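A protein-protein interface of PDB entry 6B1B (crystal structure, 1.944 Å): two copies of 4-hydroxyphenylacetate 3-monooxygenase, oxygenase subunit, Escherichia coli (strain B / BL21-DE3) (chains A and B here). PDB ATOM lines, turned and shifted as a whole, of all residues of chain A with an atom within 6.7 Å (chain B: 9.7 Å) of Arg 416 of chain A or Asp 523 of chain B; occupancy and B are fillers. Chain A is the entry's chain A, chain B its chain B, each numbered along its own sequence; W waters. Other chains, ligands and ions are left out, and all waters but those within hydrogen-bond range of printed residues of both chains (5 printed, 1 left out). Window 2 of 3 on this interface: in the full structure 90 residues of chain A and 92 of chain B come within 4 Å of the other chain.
The side-chain carboxylate (OD1) of Asp 504 of chain B lies within hydrogen-bond range of the backbone NH (N) of Gly 507 of chain B, at 3.1 Å.
The side-chain hydroxyl of Ser 257 of chain A lies within hydrogen-bond range of the side-chain carboxylate of Asp 260 of chain A, at 2.6 Å.
N of Asp 506 of chain B sits at hydrogen-bond distance from OD1 of Asp 504 of chain B, at 2.9 Å.
The side-chain amide oxygen (OD1) of Asn 520 of chain B lies within hydrogen-bond range of the backbone NH (N) of Leu 522 of chain B (3.1 Å).
The side-chain amide nitrogen (ND2) of Asn 516 of chain B lies close to the side-chain amide nitrogen (ND2) of Asn 520 of chain B (3.2 Å).
The side-chain carboxylate (OD2) of Asp 260 of chain A is in hydrogen-bond range of the backbone NH (N) of Ala 415 of chain A, at 2.9 Å.
No position is printed for both chains.
The backbone carbonyl oxygen of Gly 256 of chain A sits at hydrogen-bond distance from the side-chain amide nitrogen of Asn 520 of chain B (2.9 Å).
ND2 of Asn 516 of chain B lies within hydrogen-bond range of O of Gly 256 of chain A, 3.0 Å away.
The side-chain amide nitrogen of Gln 505 of chain B lies within hydrogen-bond range of the side-chain amide oxygen of Asn 419 of chain A (2.8 Å).
The guanidinium group (NH2) of Arg 416 of chain A is in salt-bridge range of the side-chain carboxylate (OD1) of Asp 523 of chain B (2.8 Å).
Arg 416 of chain A touches just these residues of chain B: Leu 522 and Asp 523.
Of the printed residues of chain A, Asp 523 of chain B touches Arg 416.
Ala 415 of chain A touches just one residue of chain B: Gln 505.
No residue of chain B comes within 4 Å of Asp 417 of chain A.
Of the printed residues of chain B, Ser 257 of chain A touches Asn 516 (3.8 Å).
Of the printed residues of chain A, Asp 506 of chain B touches Asn 419 (3.6 Å).
Lys 524 of chain B touches none of the printed residues of chain A.
The nearest printed residue of chain A that does not touch Asp 523 of chain B is Gly 256 of chain A (9.1 Å).
The nearest printed residue of chain B that does not touch Asn 419 of chain A is Gly 507 of chain B (6.9 Å).
Water W1 lies within hydrogen-bond range of NH1 of Arg 416 of chain A (2.6 Å) and OD1 of Asn 520 of chain B (3.0 Å).
Water W4 bridges the side-chain carboxylate (OD1) of Asp 506 of chain B and the side-chain amide oxygen (OD1) of Asn 419 of chain A.
Water W3 lies within hydrogen-bond range of the backbone carbonyl oxygen of Asp 504 of chain B (2.9 Å), the backbone NH of Tyr 259 of chain A (2.9 Å), the backbone NH of Gly 507 of chain B (3.3 Å) and the side-chain hydroxyl of Ser 257 of chain A (3.5 Å).
Water W5 lies within hydrogen-bond range of ND2 of Asn 516 of chain B (3.0 Å) and O of Gly 256 of chain A (3.5 Å).
Water W2 lies within hydrogen-bond range of the backbone carbonyl oxygen of Leu 418 of chain A and the side-chain amide nitrogen of Gln 505 of chain B.
Ser 257 of chain A touches Asn 516 of chain B.
CB of Tyr 259 of chain A touches O of Asp 504 of chain B (3.6 Å).
Tyr 259 of chain A touches Gln 505 of chain B.
CB of Ala 415 of chain A touches O of Gln 505 of chain B, at 3.5 Å.
Arg 416 of chain A touches Leu 522 of chain B (CD to CD1, 3.6 Å).
Gln 505 of chain B touches Leu 418 of chain A.
OD1 of Asp 506 of chain B touches ND2 of Asn 419 of chain A, 3.6 Å away.
Hydrophobic or aromatic side chains of chain A within 4 Å of the printed part of chain B: Tyr 259, Ala 415 and Leu 418.
Of the 14 printed residues of chain B, 7 touch a printed residue of chain A.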
ATOM      1  N   GLY A 256      -0.700  -5.636 -15.545  1.00  0.00           N
ATOM      2  CA  GLY A 256      -1.389  -5.594 -14.275  1.00  0.00           C
ATOM      3  C   GLY A 256      -2.465  -6.657 -14.227  1.00  0.00           C
ATOM      4  O   GLY A 256      -2.329  -7.715 -14.840  1.00  0.00           O
ATOM      5  N   SER A 257      -3.546  -6.367 -13.522  1.00  0.00           N
ATOM      6  CA  SER A 257      -4.655  -7.296 -13.364  1.00  0.00           C
ATOM      7  C   SER A 257      -5.857  -6.487 -12.924  1.00  0.00           C
ATOM      8  O   SER A 257      -5.711  -5.312 -12.553  1.00  0.00           O
ATOM      9  CB  SER A 257      -4.330  -8.387 -12.332  1.00  0.00           C
ATOM     10  OG  SER A 257      -4.352  -7.842 -11.023  1.00  0.00           O
ATOM     11  N   TYR A 259      -7.475  -6.880 -10.159  1.00  0.00           N
ATOM     12  CA  TYR A 259      -7.205  -6.582  -8.753  1.00  0.00           C
ATOM     13  C   TYR A 259      -6.289  -5.373  -8.601  1.00  0.00           C
ATOM     14  O   TYR A 259      -6.477  -4.550  -7.693  1.00  0.00           O
ATOM     15  CB  TYR A 259      -6.589  -7.821  -8.090  1.00  0.00           C
ATOM     16  CG  TYR A 259      -6.263  -7.696  -6.620  1.00  0.00           C
ATOM     17  CD1 TYR A 259      -5.013  -7.239  -6.221  1.00  0.00           C
ATOM     18  CD2 TYR A 259      -7.169  -8.081  -5.636  1.00  0.00           C
ATOM     19  CE1 TYR A 259      -4.682  -7.137  -4.892  1.00  0.00           C
ATOM     20  CE2 TYR A 259      -6.845  -7.984  -4.294  1.00  0.00           C
ATOM     21  CZ  TYR A 259      -5.601  -7.515  -3.931  1.00  0.00           C
ATOM     22  OH  TYR A 259      -5.289  -7.425  -2.600  1.00  0.00           O
ATOM     23  N   ASP A 260      -5.288  -5.255  -9.472  1.00  0.00           N
ATOM     24  CA  ASP A 260      -4.304  -4.179  -9.363  1.00  0.00           C
ATOM     25  C   ASP A 260      -4.792  -2.863  -9.968  1.00  0.00           C
ATOM     26  O   ASP A 260      -4.439  -1.786  -9.461  1.00  0.00           O
ATOM     27  CB  ASP A 260      -2.998  -4.629 -10.018  1.00  0.00           C
ATOM     28  CG  ASP A 260      -2.374  -5.796  -9.273  1.00  0.00           C
ATOM     29  OD1 ASP A 260      -2.040  -5.595  -8.083  1.00  0.00           O
ATOM     30  OD2 ASP A 260      -2.271  -6.906  -9.843  1.00  0.00           O
ATOM     31  N   SER A 413       3.342  -5.046  -5.640  1.00  0.00           N
ATOM     32  CA  SER A 413       3.222  -4.790  -7.073  1.00  0.00           C
ATOM     33  C   SER A 413       1.991  -5.434  -7.702  1.00  0.00           C
ATOM     34  O   SER A 413       1.476  -4.917  -8.700  1.00  0.00           O
ATOM     35  CB  SER A 413       4.476  -5.298  -7.799  1.00  0.00           C
ATOM     36  OG  SER A 413       4.566  -6.710  -7.707  1.00  0.00           O
ATOM     37  N   SER A 414       1.511  -6.556  -7.172  1.00  0.00           N
ATOM     38  CA  SER A 414       0.707  -7.404  -8.043  1.00  0.00           C
ATOM     39  C   SER A 414      -0.110  -8.416  -7.250  1.00  0.00           C
ATOM     40  O   SER A 414       0.314  -8.885  -6.194  1.00  0.00           O
ATOM     41  CB  SER A 414       1.638  -8.133  -9.031  1.00  0.00           C
ATOM     42  OG  SER A 414       0.939  -9.027  -9.862  1.00  0.00           O
ATOM     43  N   ALA A 415      -1.276  -8.783  -7.799  1.00  0.00           N
ATOM     44  CA  ALA A 415      -1.973  -9.963  -7.289  1.00  0.00           C
ATOM     45  C   ALA A 415      -1.068 -11.191  -7.327  1.00  0.00           C
ATOM     46  O   ALA A 415      -1.246 -12.117  -6.526  1.00  0.00           O
ATOM     47  CB  ALA A 415      -3.257 -10.216  -8.095  1.00  0.00           C
ATOM     48  N   ARG A 416      -0.082 -11.199  -8.235  1.00  0.00           N
ATOM     49  CA  ARG A 416       0.903 -12.278  -8.290  1.00  0.00           C
ATOM     50  C   ARG A 416       1.692 -12.409  -6.992  1.00  0.00           C
ATOM     51  O   ARG A 416       2.143 -13.513  -6.652  1.00  0.00           O
ATOM     52  CB  ARG A 416       1.865 -12.058  -9.461  1.00  0.00           C
ATOM     53  CG  ARG A 416       1.219 -12.200 -10.840  1.00  0.00           C
ATOM     54  CD  ARG A 416       2.073 -11.563 -11.940  1.00  0.00           C
ATOM     55  NE  ARG A 416       3.281 -12.333 -12.238  1.00  0.00           N
ATOM     56  CZ  ARG A 416       3.400 -13.185 -13.257  1.00  0.00           C
ATOM     57  NH1 ARG A 416       2.380 -13.393 -14.085  1.00  0.00           N
ATOM     58  NH2 ARG A 416       4.537 -13.840 -13.447  1.00  0.00           N
ATOM     59  N   ASP A 417       1.893 -11.305  -6.264  1.00  0.00           N
ATOM     60  CA  ASP A 417       2.544 -11.400  -4.958  1.00  0.00           C
ATOM     61  C   ASP A 417       1.668 -12.148  -3.955  1.00  0.00           C
ATOM     62  O   ASP A 417       2.167 -12.955  -3.160  1.00  0.00           O
ATOM     63  CB  ASP A 417       2.879 -10.003  -4.417  1.00  0.00           C
ATOM     64  CG  ASP A 417       3.826  -9.231  -5.317  1.00  0.00           C
ATOM     65  OD1 ASP A 417       4.791  -9.835  -5.840  1.00  0.00           O
ATOM     66  OD2 ASP A 417       3.609  -8.007  -5.507  1.00  0.00           O
ATOM     67  N   LEU A 418       0.358 -11.883  -3.975  1.00  0.00           N
ATOM     68  CA  LEU A 418      -0.561 -12.580  -3.079  1.00  0.00           C
ATOM     69  C   LEU A 418      -0.693 -14.050  -3.436  1.00  0.00           C
ATOM     70  O   LEU A 418      -0.981 -14.880  -2.559  1.00  0.00           O
ATOM     71  CB  LEU A 418      -1.942 -11.943  -3.142  1.00  0.00           C
ATOM     72  CG  LEU A 418      -2.039 -10.480  -2.753  1.00  0.00           C
ATOM     73  CD1 LEU A 418      -3.428  -9.993  -3.105  1.00  0.00           C
ATOM     74  CD2 LEU A 418      -1.778 -10.360  -1.264  1.00  0.00           C
ATOM     75  N   ASN A 419      -0.521 -14.387  -4.710  1.00  0.00           N
ATOM     76  CA  ASN A 419      -0.707 -15.754  -5.181  1.00  0.00           C
ATOM     77  C   ASN A 419       0.575 -16.575  -5.145  1.00  0.00           C
ATOM     78  O   ASN A 419       0.542 -17.761  -5.489  1.00  0.00           O
ATOM     79  CB  ASN A 419      -1.293 -15.740  -6.601  1.00  0.00           C
ATOM     80  CG  ASN A 419      -2.729 -15.236  -6.627  1.00  0.00           C
ATOM     81  OD1 ASN A 419      -3.469 -15.416  -5.659  1.00  0.00           O
ATOM     82  ND2 ASN A 419      -3.124 -14.581  -7.725  1.00  0.00           N
ATOM     83  N   ASN A 420       1.695 -15.977  -4.729  1.00  0.00           N
ATOM     84  CA  ASN A 420       2.932 -16.698  -4.472  1.00  0.00           C
ATOM     85  C   ASN A 420       3.082 -16.857  -2.968  1.00  0.00           C
ATOM     86  O   ASN A 420       3.379 -15.867  -2.279  1.00  0.00           O
ATOM     87  CB  ASN A 420       4.134 -15.946  -5.048  1.00  0.00           C
ATOM     88  CG  ASN A 420       5.464 -16.671  -4.804  1.00  0.00           C
ATOM     89  OD1 ASN A 420       5.556 -17.585  -3.981  1.00  0.00           O
ATOM     90  ND2 ASN A 420       6.501 -16.252  -5.522  1.00  0.00           N
ATOM     91  N   PRO A 421       2.917 -18.061  -2.416  1.00  0.00           N
ATOM     92  CA  PRO A 421       2.976 -18.206  -0.951  1.00  0.00           C
ATOM     93  C   PRO A 421       4.301 -17.777  -0.346  1.00  0.00           C
ATOM     94  O   PRO A 421       4.332 -17.424   0.837  1.00  0.00           O
ATOM     95  CB  PRO A 421       2.702 -19.705  -0.720  1.00  0.00           C
ATOM     96  CG  PRO A 421       2.805 -20.356  -2.046  1.00  0.00           C
ATOM     97  CD  PRO A 421       2.594 -19.322  -3.105  1.00  0.00           C
ATOM     98  N   ILE A 423       5.818 -15.057  -0.936  1.00  0.00           N
ATOM     99  CA  ILE A 423       5.652 -13.632  -0.644  1.00  0.00           C
ATOM    100  C   ILE A 423       4.449 -13.399   0.249  1.00  0.00           C
ATOM    101  O   ILE A 423       4.515 -12.624   1.202  1.00  0.00           O
ATOM    102  CB  ILE A 423       5.520 -12.843  -1.963  1.00  0.00           C
ATOM    103  CG1 ILE A 423       6.760 -13.038  -2.831  1.00  0.00           C
ATOM    104  CG2 ILE A 423       5.238 -11.351  -1.691  1.00  0.00           C
ATOM    105  CD1 ILE A 423       6.512 -12.764  -4.303  1.00  0.00           C
ATOM    106  N   ASP B 504     -11.451 -10.238  -7.965  1.00  0.00           N
ATOM    107  CA  ASP B 504     -10.666 -10.716  -6.832  1.00  0.00           C
ATOM    108  C   ASP B 504      -9.236 -10.924  -7.315  1.00  0.00           C
ATOM    109  O   ASP B 504      -8.895 -10.565  -8.444  1.00  0.00           O
ATOM    110  CB  ASP B 504     -11.298 -11.975  -6.218  1.00  0.00           C
ATOM    111  CG  ASP B 504     -11.393 -13.148  -7.195  1.00  0.00           C
ATOM    112  OD1 ASP B 504     -10.674 -13.188  -8.220  1.00  0.00           O
ATOM    113  OD2 ASP B 504     -12.211 -14.049  -6.923  1.00  0.00           O
ATOM    114  N   GLN B 505      -8.396 -11.533  -6.472  1.00  0.00           N
ATOM    115  CA  GLN B 505      -6.986 -11.669  -6.831  1.00  0.00           C
ATOM    116  C   GLN B 505      -6.759 -12.629  -7.990  1.00  0.00           C
ATOM    117  O   GLN B 505      -5.641 -12.687  -8.510  1.00  0.00           O
ATOM    118  CB  GLN B 505      -6.163 -12.119  -5.618  1.00  0.00           C
ATOM    119  CG  GLN B 505      -6.453 -13.549  -5.166  1.00  0.00           C
ATOM    120  CD  GLN B 505      -6.061 -13.788  -3.719  1.00  0.00           C
ATOM    121  OE1 GLN B 505      -6.840 -13.532  -2.803  1.00  0.00           O
ATOM    122  NE2 GLN B 505      -4.842 -14.280  -3.507  1.00  0.00           N
ATOM    123  N   ASP B 506      -7.787 -13.357  -8.433  1.00  0.00           N
ATOM    124  CA  ASP B 506      -7.634 -14.243  -9.582  1.00  0.00           C
ATOM    125  C   ASP B 506      -8.230 -13.682 -10.869  1.00  0.00           C
ATOM    126  O   ASP B 506      -7.984 -14.249 -11.935  1.00  0.00           O
ATOM    127  CB  ASP B 506      -8.252 -15.614  -9.282  1.00  0.00           C
ATOM    128  CG  ASP B 506      -7.543 -16.331  -8.139  1.00  0.00           C
ATOM    129  OD1 ASP B 506      -6.298 -16.245  -8.047  1.00  0.00           O
ATOM    130  OD2 ASP B 506      -8.234 -16.961  -7.319  1.00  0.00           O
ATOM    131  N   GLY B 507      -8.984 -12.582 -10.807  1.00  0.00           N
ATOM    132  CA  GLY B 507      -9.510 -11.943 -11.995  1.00  0.00           C
ATOM    133  C   GLY B 507     -10.920 -11.439 -11.763  1.00  0.00           C
ATOM    134  O   GLY B 507     -11.338 -11.213 -10.627  1.00  0.00           O
ATOM    135  N   ASN B 516      -7.691 -11.091 -18.594  1.00  0.00           N
ATOM    136  CA  ASN B 516      -6.472 -10.563 -19.209  1.00  0.00           C
ATOM    137  C   ASN B 516      -5.389 -11.626 -19.403  1.00  0.00           C
ATOM    138  O   ASN B 516      -4.278 -11.286 -19.821  1.00  0.00           O
ATOM    139  CB  ASN B 516      -5.888  -9.382 -18.397  1.00  0.00           C
ATOM    140  CG  ASN B 516      -5.250  -9.815 -17.087  1.00  0.00           C
ATOM    141  OD1 ASN B 516      -5.714 -10.747 -16.437  1.00  0.00           O
ATOM    142  ND2 ASN B 516      -4.178  -9.123 -16.687  1.00  0.00           N
ATOM    143  N   ASP B 517      -5.685 -12.901 -19.128  1.00  0.00           N
ATOM    144  CA  ASP B 517      -4.664 -13.932 -19.297  1.00  0.00           C
ATOM    145  C   ASP B 517      -4.149 -13.998 -20.728  1.00  0.00           C
ATOM    146  O   ASP B 517      -2.975 -14.310 -20.941  1.00  0.00           O
ATOM    147  CB  ASP B 517      -5.199 -15.299 -18.875  1.00  0.00           C
ATOM    148  CG  ASP B 517      -5.334 -15.422 -17.376  1.00  0.00           C
ATOM    149  OD1 ASP B 517      -5.756 -16.493 -16.891  1.00  0.00           O
ATOM    150  OD2 ASP B 517      -4.995 -14.443 -16.681  1.00  0.00           O
ATOM    151  N   ILE B 519      -3.557 -11.541 -22.717  1.00  0.00           N
ATOM    152  CA  ILE B 519      -2.720 -10.397 -23.057  1.00  0.00           C
ATOM    153  C   ILE B 519      -1.690 -10.083 -21.986  1.00  0.00           C
ATOM    154  O   ILE B 519      -0.897  -9.151 -22.158  1.00  0.00           O
ATOM    155  CB  ILE B 519      -3.567  -9.143 -23.361  1.00  0.00           C
ATOM    156  CG1 ILE B 519      -4.386  -8.715 -22.137  1.00  0.00           C
ATOM    157  CG2 ILE B 519      -4.497  -9.397 -24.537  1.00  0.00           C
ATOM    158  CD1 ILE B 519      -5.035  -7.331 -22.295  1.00  0.00           C
ATOM    159  N   ASN B 520      -1.690 -10.810 -20.878  1.00  0.00           N
ATOM    160  CA  ASN B 520      -0.774 -10.493 -19.795  1.00  0.00           C
ATOM    161  C   ASN B 520       0.638 -10.936 -20.149  1.00  0.00           C
ATOM    162  O   ASN B 520       0.867 -12.098 -20.488  1.00  0.00           O
ATOM    163  CB  ASN B 520      -1.219 -11.156 -18.502  1.00  0.00           C
ATOM    164  CG  ASN B 520      -0.487 -10.595 -17.308  1.00  0.00           C
ATOM    165  OD1 ASN B 520       0.603 -11.048 -16.978  1.00  0.00           O
ATOM    166  ND2 ASN B 520      -1.044  -9.545 -16.705  1.00  0.00           N
ATOM    167  N   MET B 521       1.584 -10.009 -20.053  1.00  0.00           N
ATOM    168  CA  MET B 521       2.945 -10.219 -20.522  1.00  0.00           C
ATOM    169  C   MET B 521       3.943 -10.444 -19.394  1.00  0.00           C
ATOM    170  O   MET B 521       5.150 -10.502 -19.657  1.00  0.00           O
ATOM    171  CB  MET B 521       3.385  -9.017 -21.362  1.00  0.00           C
ATOM    172  CG  MET B 521       2.522  -8.795 -22.594  1.00  0.00           C
ATOM    173  SD  MET B 521       2.802 -10.164 -23.731  1.00  0.00           S
ATOM    174  CE  MET B 521       1.269 -10.212 -24.646  1.00  0.00           C
ATOM    175  N   LEU B 522       3.482 -10.558 -18.147  1.00  0.00           N
ATOM    176  CA  LEU B 522       4.421 -10.557 -17.024  1.00  0.00           C
ATOM    177  C   LEU B 522       5.264 -11.836 -16.999  1.00  0.00           C
ATOM    178  O   LEU B 522       6.448 -11.798 -16.643  1.00  0.00           O
ATOM    179  CB  LEU B 522       3.661 -10.357 -15.708  1.00  0.00           C
ATOM    180  CG  LEU B 522       3.016  -8.962 -15.552  1.00  0.00           C
ATOM    181  CD1 LEU B 522       2.160  -8.872 -14.305  1.00  0.00           C
ATOM    182  CD2 LEU B 522       4.084  -7.873 -15.537  1.00  0.00           C
ATOM    183  N   ASP B 523       4.677 -12.978 -17.373  1.00  0.00           N
ATOM    184  CA  ASP B 523       5.459 -14.211 -17.470  1.00  0.00           C
ATOM    185  C   ASP B 523       6.612 -14.057 -18.458  1.00  0.00           C
ATOM    186  O   ASP B 523       7.765 -14.376 -18.140  1.00  0.00           O
ATOM    187  CB  ASP B 523       4.564 -15.381 -17.883  1.00  0.00           C
ATOM    188  CG  ASP B 523       3.768 -15.944 -16.725  1.00  0.00           C
ATOM    189  OD1 ASP B 523       3.997 -15.519 -15.573  1.00  0.00           O
ATOM    190  OD2 ASP B 523       2.929 -16.837 -16.971  1.00  0.00           O
ATOM    191  N   LYS B 524       6.315 -13.569 -19.668  1.00  0.00           N
ATOM    192  CA  LYS B 524       7.364 -13.324 -20.656  1.00  0.00           C
ATOM    193  C   LYS B 524       8.447 -12.400 -20.120  1.00  0.00           C
ATOM    194  O   LYS B 524       9.640 -12.635 -20.338  1.00  0.00           O
ATOM    195  CB  LYS B 524       6.766 -12.707 -21.917  1.00  0.00           C
ATOM    196  CG  LYS B 524       5.881 -13.581 -22.761  1.00  0.00           C
ATOM    197  CD  LYS B 524       5.510 -12.807 -24.022  1.00  0.00           C
ATOM    198  CE  LYS B 524       5.014 -13.713 -25.129  1.00  0.00           C
ATOM    199  NZ  LYS B 524       4.884 -15.117 -24.668  1.00  0.00           N
ATOM    200  N   LEU B 525       8.048 -11.335 -19.430  1.00  0.00           N
ATOM    201  CA  LEU B 525       9.017 -10.347 -18.977  1.00  0.00           C
ATOM    202  C   LEU B 525       9.906 -10.883 -17.872  1.00  0.00           C
ATOM    203  O   LEU B 525      11.059 -10.458 -17.746  1.00  0.00           O
ATOM    204  CB  LEU B 525       8.298  -9.094 -18.480  1.00  0.00           C
ATOM    205  CG  LEU B 525       7.816  -8.160 -19.578  1.00  0.00           C
ATOM    206  CD1 LEU B 525       6.756  -7.196 -19.027  1.00  0.00           C
ATOM    207  CD2 LEU B 525       9.009  -7.414 -20.140  1.00  0.00           C
ATOM    208  N   LEU B 526       9.389 -11.777 -17.043  1.00  0.00           N
ATOM    209  CA  LEU B 526      10.086 -12.113 -15.819  1.00  0.00           C
ATOM    210  C   LEU B 526      10.563 -13.555 -15.787  1.00  0.00           C
ATOM    211  O   LEU B 526      11.260 -13.934 -14.852  1.00  0.00           O
ATOM    212  CB  LEU B 526       9.180 -11.838 -14.628  1.00  0.00           C
ATOM    213  CG  LEU B 526       8.636 -10.413 -14.653  1.00  0.00           C
ATOM    214  CD1 LEU B 526       7.615 -10.257 -13.576  1.00  0.00           C
ATOM    215  CD2 LEU B 526       9.777  -9.404 -14.470  1.00  0.00           C
HETATM  216  O   HOH W   1       0.085 -12.262 -14.259  1.00  0.00           O
HETATM  217  O   HOH W   2      -3.447 -14.437  -0.711  1.00  0.00           O
HETATM  218  O   HOH W   3      -7.227  -9.762 -10.635  1.00  0.00           O
HETATM  219  O   HOH W   4      -5.679 -17.131  -5.503  1.00  0.00           O
HETATM  220  O   HOH W   5      -3.468 -10.973 -14.431  1.00  0.00           O
